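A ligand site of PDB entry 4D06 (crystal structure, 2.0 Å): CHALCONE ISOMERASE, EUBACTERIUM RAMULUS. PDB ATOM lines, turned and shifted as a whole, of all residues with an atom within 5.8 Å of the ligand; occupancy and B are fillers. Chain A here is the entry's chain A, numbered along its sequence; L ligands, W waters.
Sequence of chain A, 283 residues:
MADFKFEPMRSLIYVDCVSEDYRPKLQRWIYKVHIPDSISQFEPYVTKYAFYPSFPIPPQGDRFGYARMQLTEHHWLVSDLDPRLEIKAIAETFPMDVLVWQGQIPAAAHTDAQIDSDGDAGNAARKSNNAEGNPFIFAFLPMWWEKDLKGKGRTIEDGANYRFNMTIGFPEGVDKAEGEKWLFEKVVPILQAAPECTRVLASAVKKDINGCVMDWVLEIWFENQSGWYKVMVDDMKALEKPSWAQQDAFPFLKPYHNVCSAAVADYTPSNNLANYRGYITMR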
ATOM      1  N   ILE A  13       1.352 -22.339 -19.851  1.00  0.00           N
ATOM      2  CA  ILE A  13       2.255 -21.249 -20.130  1.00  0.00           C
ATOM      3  C   ILE A  13       1.474 -20.088 -20.712  1.00  0.00           C
ATOM      4  O   ILE A  13       0.653 -20.265 -21.609  1.00  0.00           O
ATOM      5  CB  ILE A  13       3.295 -21.705 -21.151  1.00  0.00           C
ATOM      6  CG1 ILE A  13       4.220 -22.736 -20.511  1.00  0.00           C
ATOM      7  CG2 ILE A  13       4.131 -20.530 -21.669  1.00  0.00           C
ATOM      8  CD1 ILE A  13       5.034 -23.485 -21.502  1.00  0.00           C
ATOM      9  N   VAL A  15       1.473 -16.944 -22.837  1.00  0.00           N
ATOM     10  CA  VAL A  15       2.255 -16.421 -23.966  1.00  0.00           C
ATOM     11  C   VAL A  15       1.724 -15.071 -24.440  1.00  0.00           C
ATOM     12  O   VAL A  15       0.655 -14.988 -25.073  1.00  0.00           O
ATOM     13  CB  VAL A  15       2.224 -17.364 -25.149  1.00  0.00           C
ATOM     14  CG1 VAL A  15       3.151 -16.853 -26.195  1.00  0.00           C
ATOM     15  CG2 VAL A  15       2.692 -18.742 -24.746  1.00  0.00           C
ATOM     16  N   TRP A  29       7.016 -18.386 -35.612  1.00  0.00           N
ATOM     17  CA  TRP A  29       7.962 -19.231 -34.875  1.00  0.00           C
ATOM     18  C   TRP A  29       7.186 -20.381 -34.154  1.00  0.00           C
ATOM     19  O   TRP A  29       7.597 -21.550 -34.205  1.00  0.00           O
ATOM     20  CB  TRP A  29       8.787 -18.411 -33.890  1.00  0.00           C
ATOM     21  CG  TRP A  29       9.696 -19.256 -33.053  1.00  0.00           C
ATOM     22  CD1 TRP A  29      10.894 -19.779 -33.382  1.00  0.00           C
ATOM     23  CD2 TRP A  29       9.417 -19.703 -31.749  1.00  0.00           C
ATOM     24  NE1 TRP A  29      11.406 -20.559 -32.339  1.00  0.00           N
ATOM     25  CE2 TRP A  29      10.500 -20.536 -31.335  1.00  0.00           C
ATOM     26  CE3 TRP A  29       8.355 -19.505 -30.883  1.00  0.00           C
ATOM     27  CZ2 TRP A  29      10.531 -21.155 -30.079  1.00  0.00           C
ATOM     28  CZ3 TRP A  29       8.407 -20.102 -29.604  1.00  0.00           C
ATOM     29  CH2 TRP A  29       9.498 -20.909 -29.237  1.00  0.00           C
ATOM     30  N   ILE A  30       6.119 -20.008 -33.479  1.00  0.00           N
ATOM     31  CA  ILE A  30       5.315 -20.969 -32.720  1.00  0.00           C
ATOM     32  C   ILE A  30       4.867 -22.148 -33.611  1.00  0.00           C
ATOM     33  O   ILE A  30       5.144 -23.319 -33.258  1.00  0.00           O
ATOM     34  CB  ILE A  30       4.124 -20.273 -32.043  1.00  0.00           C
ATOM     35  CG1 ILE A  30       4.608 -19.466 -30.850  1.00  0.00           C
ATOM     36  CG2 ILE A  30       3.128 -21.308 -31.556  1.00  0.00           C
ATOM     37  CD1 ILE A  30       3.568 -18.546 -30.266  1.00  0.00           C
ATOM     38  N   HIS A  34       8.484 -24.165 -33.695  1.00  0.00           N
ATOM     39  CA  HIS A  34       8.452 -24.695 -32.360  1.00  0.00           C
ATOM     40  C   HIS A  34       7.643 -25.985 -32.184  1.00  0.00           C
ATOM     41  O   HIS A  34       8.044 -26.876 -31.432  1.00  0.00           O
ATOM     42  CB  HIS A  34       7.967 -23.648 -31.421  1.00  0.00           C
ATOM     43  CG  HIS A  34       8.259 -23.972 -30.000  1.00  0.00           C
ATOM     44  ND1 HIS A  34       9.526 -24.360 -29.598  1.00  0.00           N
ATOM     45  CD2 HIS A  34       7.481 -24.032 -28.909  1.00  0.00           C
ATOM     46  CE1 HIS A  34       9.527 -24.571 -28.299  1.00  0.00           C
ATOM     47  NE2 HIS A  34       8.292 -24.406 -27.866  1.00  0.00           N
ATOM     48  N   SER A  38       9.101 -29.413 -30.434  1.00  0.00           N
ATOM     49  CA  SER A  38       8.506 -29.799 -29.160  1.00  0.00           C
ATOM     50  C   SER A  38       7.933 -31.192 -29.259  1.00  0.00           C
ATOM     51  O   SER A  38       8.150 -32.043 -28.370  1.00  0.00           O
ATOM     52  CB  SER A  38       7.402 -28.849 -28.797  1.00  0.00           C
ATOM     53  OG  SER A  38       7.937 -27.575 -28.580  1.00  0.00           O
ATOM     54  N   GLN A  41      10.677 -33.768 -29.192  1.00  0.00           N
ATOM     55  CA  GLN A  41      11.258 -34.019 -27.877  1.00  0.00           C
ATOM     56  C   GLN A  41      10.385 -34.880 -26.958  1.00  0.00           C
ATOM     57  O   GLN A  41      10.846 -35.878 -26.295  1.00  0.00           O
ATOM     58  CB  GLN A  41      11.521 -32.697 -27.163  1.00  0.00           C
ATOM     59  CG  GLN A  41      12.546 -31.797 -27.809  1.00  0.00           C
ATOM     60  CD  GLN A  41      12.976 -30.633 -26.945  1.00  0.00           C
ATOM     61  OE1 GLN A  41      12.611 -30.511 -25.768  1.00  0.00           O
ATOM     62  NE2 GLN A  41      13.862 -29.838 -27.476  1.00  0.00           N
ATOM     63  N   PHE A  42       9.108 -34.528 -26.895  1.00  0.00           N
ATOM     64  CA  PHE A  42       8.250 -35.161 -25.863  1.00  0.00           C
ATOM     65  C   PHE A  42       7.071 -36.007 -26.270  1.00  0.00           C
ATOM     66  O   PHE A  42       6.271 -36.463 -25.427  1.00  0.00           O
ATOM     67  CB  PHE A  42       7.816 -34.079 -24.884  1.00  0.00           C
ATOM     68  CG  PHE A  42       7.016 -32.932 -25.494  1.00  0.00           C
ATOM     69  CD1 PHE A  42       5.895 -33.136 -26.233  1.00  0.00           C
ATOM     70  CD2 PHE A  42       7.353 -31.644 -25.146  1.00  0.00           C
ATOM     71  CE1 PHE A  42       5.138 -32.062 -26.705  1.00  0.00           C
ATOM     72  CE2 PHE A  42       6.636 -30.552 -25.591  1.00  0.00           C
ATOM     73  CZ  PHE A  42       5.491 -30.768 -26.374  1.00  0.00           C
ATOM     74  N   TYR A  49      -0.844 -31.780 -26.236  1.00  0.00           N
ATOM     75  CA  TYR A  49      -0.089 -30.580 -26.369  1.00  0.00           C
ATOM     76  C   TYR A  49      -0.951 -29.659 -27.238  1.00  0.00           C
ATOM     77  O   TYR A  49      -1.225 -29.996 -28.396  1.00  0.00           O
ATOM     78  CB  TYR A  49       1.210 -30.913 -27.087  1.00  0.00           C
ATOM     79  CG  TYR A  49       2.061 -29.800 -27.555  1.00  0.00           C
ATOM     80  CD1 TYR A  49       2.303 -28.703 -26.764  1.00  0.00           C
ATOM     81  CD2 TYR A  49       2.755 -29.884 -28.741  1.00  0.00           C
ATOM     82  CE1 TYR A  49       3.156 -27.675 -27.151  1.00  0.00           C
ATOM     83  CE2 TYR A  49       3.597 -28.856 -29.168  1.00  0.00           C
ATOM     84  CZ  TYR A  49       3.784 -27.756 -28.369  1.00  0.00           C
ATOM     85  OH  TYR A  49       4.651 -26.748 -28.791  1.00  0.00           O
ATOM     86  N   PHE A  51      -2.601 -25.449 -28.035  1.00  0.00           N
ATOM     87  CA  PHE A  51      -2.572 -23.995 -27.904  1.00  0.00           C
ATOM     88  C   PHE A  51      -3.999 -23.440 -27.974  1.00  0.00           C
ATOM     89  O   PHE A  51      -4.772 -23.866 -28.836  1.00  0.00           O
ATOM     90  CB  PHE A  51      -1.788 -23.328 -29.071  1.00  0.00           C
ATOM     91  CG  PHE A  51      -0.402 -23.844 -29.302  1.00  0.00           C
ATOM     92  CD1 PHE A  51       0.417 -24.222 -28.294  1.00  0.00           C
ATOM     93  CD2 PHE A  51       0.132 -23.785 -30.600  1.00  0.00           C
ATOM     94  CE1 PHE A  51       1.749 -24.573 -28.533  1.00  0.00           C
ATOM     95  CE2 PHE A  51       1.444 -24.189 -30.850  1.00  0.00           C
ATOM     96  CZ  PHE A  51       2.262 -24.561 -29.834  1.00  0.00           C
ATOM     97  N   GLN A  70      -1.437 -16.480 -26.585  1.00  0.00           N
ATOM     98  CA  GLN A  70      -2.145 -17.752 -26.327  1.00  0.00           C
ATOM     99  C   GLN A  70      -1.832 -18.319 -24.967  1.00  0.00           C
ATOM    100  O   GLN A  70      -0.876 -17.916 -24.307  1.00  0.00           O
ATOM    101  CB  GLN A  70      -1.765 -18.771 -27.411  1.00  0.00           C
ATOM    102  CG  GLN A  70      -0.336 -19.297 -27.234  1.00  0.00           C
ATOM    103  CD  GLN A  70       0.186 -20.011 -28.465  1.00  0.00           C
ATOM    104  OE1 GLN A  70      -0.015 -19.560 -29.584  1.00  0.00           O
ATOM    105  NE2 GLN A  70       0.936 -21.089 -28.260  1.00  0.00           N
ATOM    106  N   THR A  72      -0.472 -21.950 -23.690  1.00  0.00           N
ATOM    107  CA  THR A  72       0.069 -23.219 -24.140  1.00  0.00           C
ATOM    108  C   THR A  72      -0.124 -24.279 -23.045  1.00  0.00           C
ATOM    109  O   THR A  72       0.229 -24.059 -21.890  1.00  0.00           O
ATOM    110  CB  THR A  72       1.546 -23.055 -24.463  1.00  0.00           C
ATOM    111  OG1 THR A  72       1.716 -22.231 -25.652  1.00  0.00           O
ATOM    112  CG2 THR A  72       2.238 -24.410 -24.629  1.00  0.00           C
ATOM    113  N   HIS A  74       0.245 -28.393 -21.826  1.00  0.00           N
ATOM    114  CA  HIS A  74       0.790 -29.740 -21.944  1.00  0.00           C
ATOM    115  C   HIS A  74       0.121 -30.631 -20.898  1.00  0.00           C
ATOM    116  O   HIS A  74      -0.148 -30.171 -19.782  1.00  0.00           O
ATOM    117  CB  HIS A  74       2.289 -29.763 -21.615  1.00  0.00           C
ATOM    118  CG  HIS A  74       3.163 -28.991 -22.578  1.00  0.00           C
ATOM    119  ND1 HIS A  74       3.216 -27.624 -22.581  1.00  0.00           N
ATOM    120  CD2 HIS A  74       4.035 -29.415 -23.532  1.00  0.00           C
ATOM    121  CE1 HIS A  74       4.092 -27.225 -23.489  1.00  0.00           C
ATOM    122  NE2 HIS A  74       4.583 -28.299 -24.098  1.00  0.00           N
ATOM    123  N   TRP A  76       1.501 -33.965 -19.088  1.00  0.00           N
ATOM    124  CA  TRP A  76       2.752 -34.683 -18.896  1.00  0.00           C
ATOM    125  C   TRP A  76       2.501 -35.965 -18.153  1.00  0.00           C
ATOM    126  O   TRP A  76       1.639 -36.008 -17.260  1.00  0.00           O
ATOM    127  CB  TRP A  76       3.718 -33.864 -18.005  1.00  0.00           C
ATOM    128  CG  TRP A  76       4.036 -32.499 -18.516  1.00  0.00           C
ATOM    129  CD1 TRP A  76       3.393 -31.358 -18.200  1.00  0.00           C
ATOM    130  CD2 TRP A  76       5.135 -32.136 -19.330  1.00  0.00           C
ATOM    131  NE1 TRP A  76       3.989 -30.311 -18.811  1.00  0.00           N
ATOM    132  CE2 TRP A  76       5.047 -30.776 -19.541  1.00  0.00           C
ATOM    133  CE3 TRP A  76       6.165 -32.861 -19.943  1.00  0.00           C
ATOM    134  CZ2 TRP A  76       5.924 -30.087 -20.386  1.00  0.00           C
ATOM    135  CZ3 TRP A  76       7.025 -32.211 -20.796  1.00  0.00           C
ATOM    136  CH2 TRP A  76       6.908 -30.794 -21.003  1.00  0.00           C
ATOM    137  N   ASP A  80       8.911 -32.696 -16.375  1.00  0.00           N
ATOM    138  CA  ASP A  80       9.844 -32.131 -17.349  1.00  0.00           C
ATOM    139  C   ASP A  80      11.087 -31.546 -16.689  1.00  0.00           C
ATOM    140  O   ASP A  80      12.044 -31.196 -17.373  1.00  0.00           O
ATOM    141  CB  ASP A  80       9.153 -31.020 -18.168  1.00  0.00           C
ATOM    142  CG  ASP A  80       9.984 -30.573 -19.437  1.00  0.00           C
ATOM    143  OD1 ASP A  80      10.533 -31.437 -20.122  1.00  0.00           O
ATOM    144  OD2 ASP A  80       9.970 -29.354 -19.736  1.00  0.00           O
ATOM    145  N   LYS A  88      18.956 -33.792 -24.567  1.00  0.00           N
ATOM    146  CA  LYS A  88      18.111 -33.824 -25.775  1.00  0.00           C
ATOM    147  C   LYS A  88      18.970 -33.985 -27.017  1.00  0.00           C
ATOM    148  O   LYS A  88      19.917 -33.212 -27.181  1.00  0.00           O
ATOM    149  CB  LYS A  88      17.263 -32.530 -25.928  1.00  0.00           C
ATOM    150  CG  LYS A  88      16.355 -32.283 -24.706  1.00  0.00           C
ATOM    151  CD  LYS A  88      15.739 -30.893 -24.640  1.00  0.00           C
ATOM    152  CE  LYS A  88      14.845 -30.778 -23.389  1.00  0.00           C
ATOM    153  NZ  LYS A  88      13.956 -29.552 -23.361  1.00  0.00           N
ATOM    154  N   GLU A  92      15.885 -27.271 -29.104  1.00  0.00           N
ATOM    155  CA  GLU A  92      14.965 -26.381 -29.733  1.00  0.00           C
ATOM    156  C   GLU A  92      15.661 -25.207 -30.452  1.00  0.00           C
ATOM    157  O   GLU A  92      16.591 -24.650 -29.918  1.00  0.00           O
ATOM    158  CB  GLU A  92      14.056 -25.745 -28.682  1.00  0.00           C
ATOM    159  CG  GLU A  92      13.082 -26.706 -28.087  1.00  0.00           C
ATOM    160  CD  GLU A  92      12.781 -26.406 -26.575  1.00  0.00           C
ATOM    161  OE1 GLU A  92      12.185 -25.278 -26.335  1.00  0.00           O
ATOM    162  OE2 GLU A  92      13.166 -27.268 -25.692  1.00  0.00           O
ATOM    163  N   PHE A  94      15.563 -21.705 -30.893  1.00  0.00           N
ATOM    164  CA  PHE A  94      14.948 -20.750 -29.990  1.00  0.00           C
ATOM    165  C   PHE A  94      15.784 -19.483 -30.044  1.00  0.00           C
ATOM    166  O   PHE A  94      16.694 -19.327 -29.227  1.00  0.00           O
ATOM    167  CB  PHE A  94      14.943 -21.249 -28.564  1.00  0.00           C
ATOM    168  CG  PHE A  94      13.714 -20.858 -27.733  1.00  0.00           C
ATOM    169  CD1 PHE A  94      13.436 -19.560 -27.458  1.00  0.00           C
ATOM    170  CD2 PHE A  94      12.893 -21.880 -27.131  1.00  0.00           C
ATOM    171  CE1 PHE A  94      12.389 -19.188 -26.652  1.00  0.00           C
ATOM    172  CE2 PHE A  94      11.791 -21.531 -26.299  1.00  0.00           C
ATOM    173  CZ  PHE A  94      11.545 -20.151 -26.073  1.00  0.00           C
ATOM    174  N   VAL A  98      12.385 -14.438 -29.591  1.00  0.00           N
ATOM    175  CA  VAL A  98      11.115 -14.892 -29.061  1.00  0.00           C
ATOM    176  C   VAL A  98      10.854 -14.266 -27.692  1.00  0.00           C
ATOM    177  O   VAL A  98       9.723 -13.866 -27.364  1.00  0.00           O
ATOM    178  CB  VAL A  98      11.119 -16.426 -28.896  1.00  0.00           C
ATOM    179  CG1 VAL A  98       9.879 -16.886 -28.115  1.00  0.00           C
ATOM    180  CG2 VAL A  98      11.092 -17.059 -30.263  1.00  0.00           C
ATOM    181  N   GLN A 102       7.653 -11.842 -26.729  1.00  0.00           N
ATOM    182  CA  GLN A 102       6.752 -12.203 -25.647  1.00  0.00           C
ATOM    183  C   GLN A 102       6.871 -11.241 -24.461  1.00  0.00           C
ATOM    184  O   GLN A 102       6.087 -11.332 -23.499  1.00  0.00           O
ATOM    185  CB  GLN A 102       7.018 -13.632 -25.165  1.00  0.00           C
ATOM    186  CG  GLN A 102       6.682 -14.680 -26.206  1.00  0.00           C
ATOM    187  CD  GLN A 102       6.983 -16.121 -25.788  1.00  0.00           C
ATOM    188  OE1 GLN A 102       6.708 -17.056 -26.545  1.00  0.00           O
ATOM    189  NE2 GLN A 102       7.608 -16.295 -24.660  1.00  0.00           N
ATOM    190  N   GLN A 104       9.578 -11.022 -22.275  1.00  0.00           N
ATOM    191  CA  GLN A 104      10.542 -11.426 -21.237  1.00  0.00           C
ATOM    192  C   GLN A 104      11.786 -10.481 -21.199  1.00  0.00           C
ATOM    193  O   GLN A 104      12.338 -10.249 -20.107  1.00  0.00           O
ATOM    194  CB  GLN A 104      11.004 -12.865 -21.452  1.00  0.00           C
ATOM    195  CG  GLN A 104      10.117 -13.933 -20.843  1.00  0.00           C
ATOM    196  CD  GLN A 104       8.874 -14.146 -21.609  1.00  0.00           C
ATOM    197  OE1 GLN A 104       8.924 -14.511 -22.776  1.00  0.00           O
ATOM    198  NE2 GLN A 104       7.723 -13.940 -20.972  1.00  0.00           N
ATOM    199  N   ASN A 123      14.827 -25.012 -21.970  1.00  0.00           N
ATOM    200  CA  ASN A 123      14.542 -25.057 -20.514  1.00  0.00           C
ATOM    201  C   ASN A 123      14.938 -23.717 -19.806  1.00  0.00           C
ATOM    202  O   ASN A 123      14.169 -23.184 -18.947  1.00  0.00           O
ATOM    203  CB  ASN A 123      15.202 -26.286 -19.847  1.00  0.00           C
ATOM    204  CG  ASN A 123      14.471 -27.612 -20.137  1.00  0.00           C
ATOM    205  OD1 ASN A 123      13.421 -27.647 -20.790  1.00  0.00           O
ATOM    206  ND2 ASN A 123      15.060 -28.718 -19.663  1.00  0.00           N
ATOM    207  N   ARG A 126      12.414 -20.908 -20.778  1.00  0.00           N
ATOM    208  CA  ARG A 126      11.208 -21.134 -19.953  1.00  0.00           C
ATOM    209  C   ARG A 126      11.361 -20.751 -18.441  1.00  0.00           C
ATOM    210  O   ARG A 126      10.365 -20.710 -17.688  1.00  0.00           O
ATOM    211  CB  ARG A 126      10.697 -22.609 -20.123  1.00  0.00           C
ATOM    212  CG  ARG A 126      10.091 -22.872 -21.528  1.00  0.00           C
ATOM    213  CD  ARG A 126       9.482 -24.256 -21.687  1.00  0.00           C
ATOM    214  NE  ARG A 126      10.533 -25.262 -21.893  1.00  0.00           N
ATOM    215  CZ  ARG A 126      11.159 -25.474 -23.058  1.00  0.00           C
ATOM    216  NH1 ARG A 126      10.790 -24.742 -24.169  1.00  0.00           N
ATOM    217  NH2 ARG A 126      12.153 -26.412 -23.104  1.00  0.00           N
ATOM    218  N   PHE A 136       8.909 -15.504 -17.437  1.00  0.00           N
ATOM    219  CA  PHE A 136       8.255 -16.564 -18.154  1.00  0.00           C
ATOM    220  C   PHE A 136       7.452 -17.368 -17.122  1.00  0.00           C
ATOM    221  O   PHE A 136       8.038 -17.939 -16.217  1.00  0.00           O
ATOM    222  CB  PHE A 136       9.290 -17.462 -18.781  1.00  0.00           C
ATOM    223  CG  PHE A 136       8.725 -18.405 -19.780  1.00  0.00           C
ATOM    224  CD1 PHE A 136       8.263 -19.620 -19.398  1.00  0.00           C
ATOM    225  CD2 PHE A 136       8.697 -18.068 -21.104  1.00  0.00           C
ATOM    226  CE1 PHE A 136       7.725 -20.500 -20.317  1.00  0.00           C
ATOM    227  CE2 PHE A 136       8.154 -18.956 -22.055  1.00  0.00           C
ATOM    228  CZ  PHE A 136       7.652 -20.169 -21.640  1.00  0.00           C
ATOM    229  N   PHE A 138       5.267 -20.515 -16.195  1.00  0.00           N
ATOM    230  CA  PHE A 138       5.058 -21.901 -16.598  1.00  0.00           C
ATOM    231  C   PHE A 138       4.577 -22.601 -15.321  1.00  0.00           C
ATOM    232  O   PHE A 138       5.377 -22.872 -14.426  1.00  0.00           O
ATOM    233  CB  PHE A 138       6.410 -22.406 -17.059  1.00  0.00           C
ATOM    234  CG  PHE A 138       6.475 -23.819 -17.602  1.00  0.00           C
ATOM    235  CD1 PHE A 138       5.381 -24.565 -17.919  1.00  0.00           C
ATOM    236  CD2 PHE A 138       7.733 -24.365 -17.857  1.00  0.00           C
ATOM    237  CE1 PHE A 138       5.512 -25.856 -18.441  1.00  0.00           C
ATOM    238  CE2 PHE A 138       7.879 -25.668 -18.369  1.00  0.00           C
ATOM    239  CZ  PHE A 138       6.747 -26.405 -18.695  1.00  0.00           C
HETATM  240  C1  LIG L   1       7.765 -21.598 -25.145  1.00  0.00           C
HETATM  241  C2  LIG L   1       7.070 -20.487 -25.656  1.00  0.00           C
HETATM  242  C3  LIG L   1       5.844 -20.589 -26.305  1.00  0.00           C
HETATM  243  C4  LIG L   1       5.277 -21.874 -26.451  1.00  0.00           C
HETATM  244  C5  LIG L   1       5.977 -23.052 -25.937  1.00  0.00           C
HETATM  245  C6  LIG L   1       7.293 -22.881 -25.287  1.00  0.00           C
HETATM  246  C7  LIG L   1       5.481 -24.442 -26.213  1.00  0.00           C
HETATM  247  C8  LIG L   1       6.183 -25.650 -25.650  1.00  0.00           C
HETATM  248  C9  LIG L   1       7.033 -25.228 -24.473  1.00  0.00           C
HETATM  249  O1  LIG L   1       7.907 -24.053 -24.848  1.00  0.00           O
HETATM  250  O2  LIG L   1       4.673 -24.614 -27.114  1.00  0.00           O
HETATM  251  C10 LIG L   1       7.842 -26.397 -23.921  1.00  0.00           C
HETATM  252  C11 LIG L   1       7.875 -26.694 -22.577  1.00  0.00           C
HETATM  253  C12 LIG L   1       8.695 -27.698 -22.081  1.00  0.00           C
HETATM  254  C13 LIG L   1       9.467 -28.454 -22.915  1.00  0.00           C
HETATM  255  C14 LIG L   1       9.442 -28.192 -24.282  1.00  0.00           C
HETATM  256  C15 LIG L   1       8.634 -27.177 -24.774  1.00  0.00           C
HETATM  257  O3  LIG L   1      10.293 -29.419 -22.488  1.00  0.00           O
HETATM  258  O4  LIG L   1       7.638 -19.276 -25.502  1.00  0.00           O
HETATM  259  O5  LIG L   1       4.138 -22.114 -27.073  1.00  0.00           O
HETATM  260  O   HOH W   1      10.878 -32.707 -22.342  1.00  0.00           O
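OG1 of Thr 72 is in hydrogen-bond range of O5 of the ligand (2.8 Å). The side-chain hydroxyl (OH) of Tyr 49 lies within hydrogen-bond range of an oxygen (O2) of the ligand (2.7 Å). An oxygen (O4) of the ligand lies close to the side-chain amide oxygen of Gln 102, 2.6 Å away. An oxygen (O1) of the ligand sits at hydrogen-bond distance from a ring nitrogen (NE2) of His 34, at 3.1 Å. O1 of the ligand lies within hydrogen-bond range of NH1 of Arg 126 (3.0 Å). O3 of the ligand sits at hydrogen-bond distance from OD2 of Asp 80 (2.8 Å).
The side-chain amino group (NZ) of Lys 88 lies within hydrogen-bond range of the side-chain amide oxygen (OD1) of Asn 123 (3.2 Å). The backbone carbonyl oxygen of His 34 is in hydrogen-bond range of the side-chain hydroxyl of Ser 38. NH2 of Arg 126 lies within hydrogen-bond range of OD1 of Asn 123 (2.9 Å). The side-chain amide nitrogen (NE2) of Gln 70 sits at hydrogen-bond distance from the side-chain hydroxyl (OG1) of Thr 72 (3.0 Å). NZ of Lys 88 lies within salt-bridge range of OE2 of Glu 92 (3.4 Å). The backbone NH (N) of His 34 lies within hydrogen-bond range of the backbone carbonyl oxygen (O) of Trp 29 (2.8 Å). O of Thr 72 sits at hydrogen-bond distance from N of Ile 13. OG of Ser 38 lies within hydrogen-bond range of OH of Tyr 49, 3.4 Å away.
Ile 13 touches the ligand (CD1 to C9, 3.98 Å). Val 15 touches the ligand (CG2 to C3, 3.97 Å). Ser 38 touches the ligand. Phe 42 touches the ligand. Phe 51 touches the ligand (CE1 to O2, 3.3 Å). Gln 70 touches the ligand. CE1 of His 74 touches C8 of the ligand (3.4 Å). Trp 76 touches the ligand. Lys 88 touches the ligand (NZ to O3, 3.8 Å). Asn 123 touches the ligand. CE2 of Phe 136 touches O4 of the ligand (3.5 Å). 17 residues have an atom within 4 Å of the ligand: Ile 13, Val 15, His 34, Ser 38, Phe 42, Tyr 49, Phe 51, Gln 70, Thr 72, His 74, Trp 76, Asp 80, Lys 88, Gln 102, Asn 123, Arg 126 and Phe 136. The nearest printed residue that does not touch the ligand is Phe 94 (4.04 Å).
Water W1 bridges OD1 of Asp 80 and O3 of the ligand.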
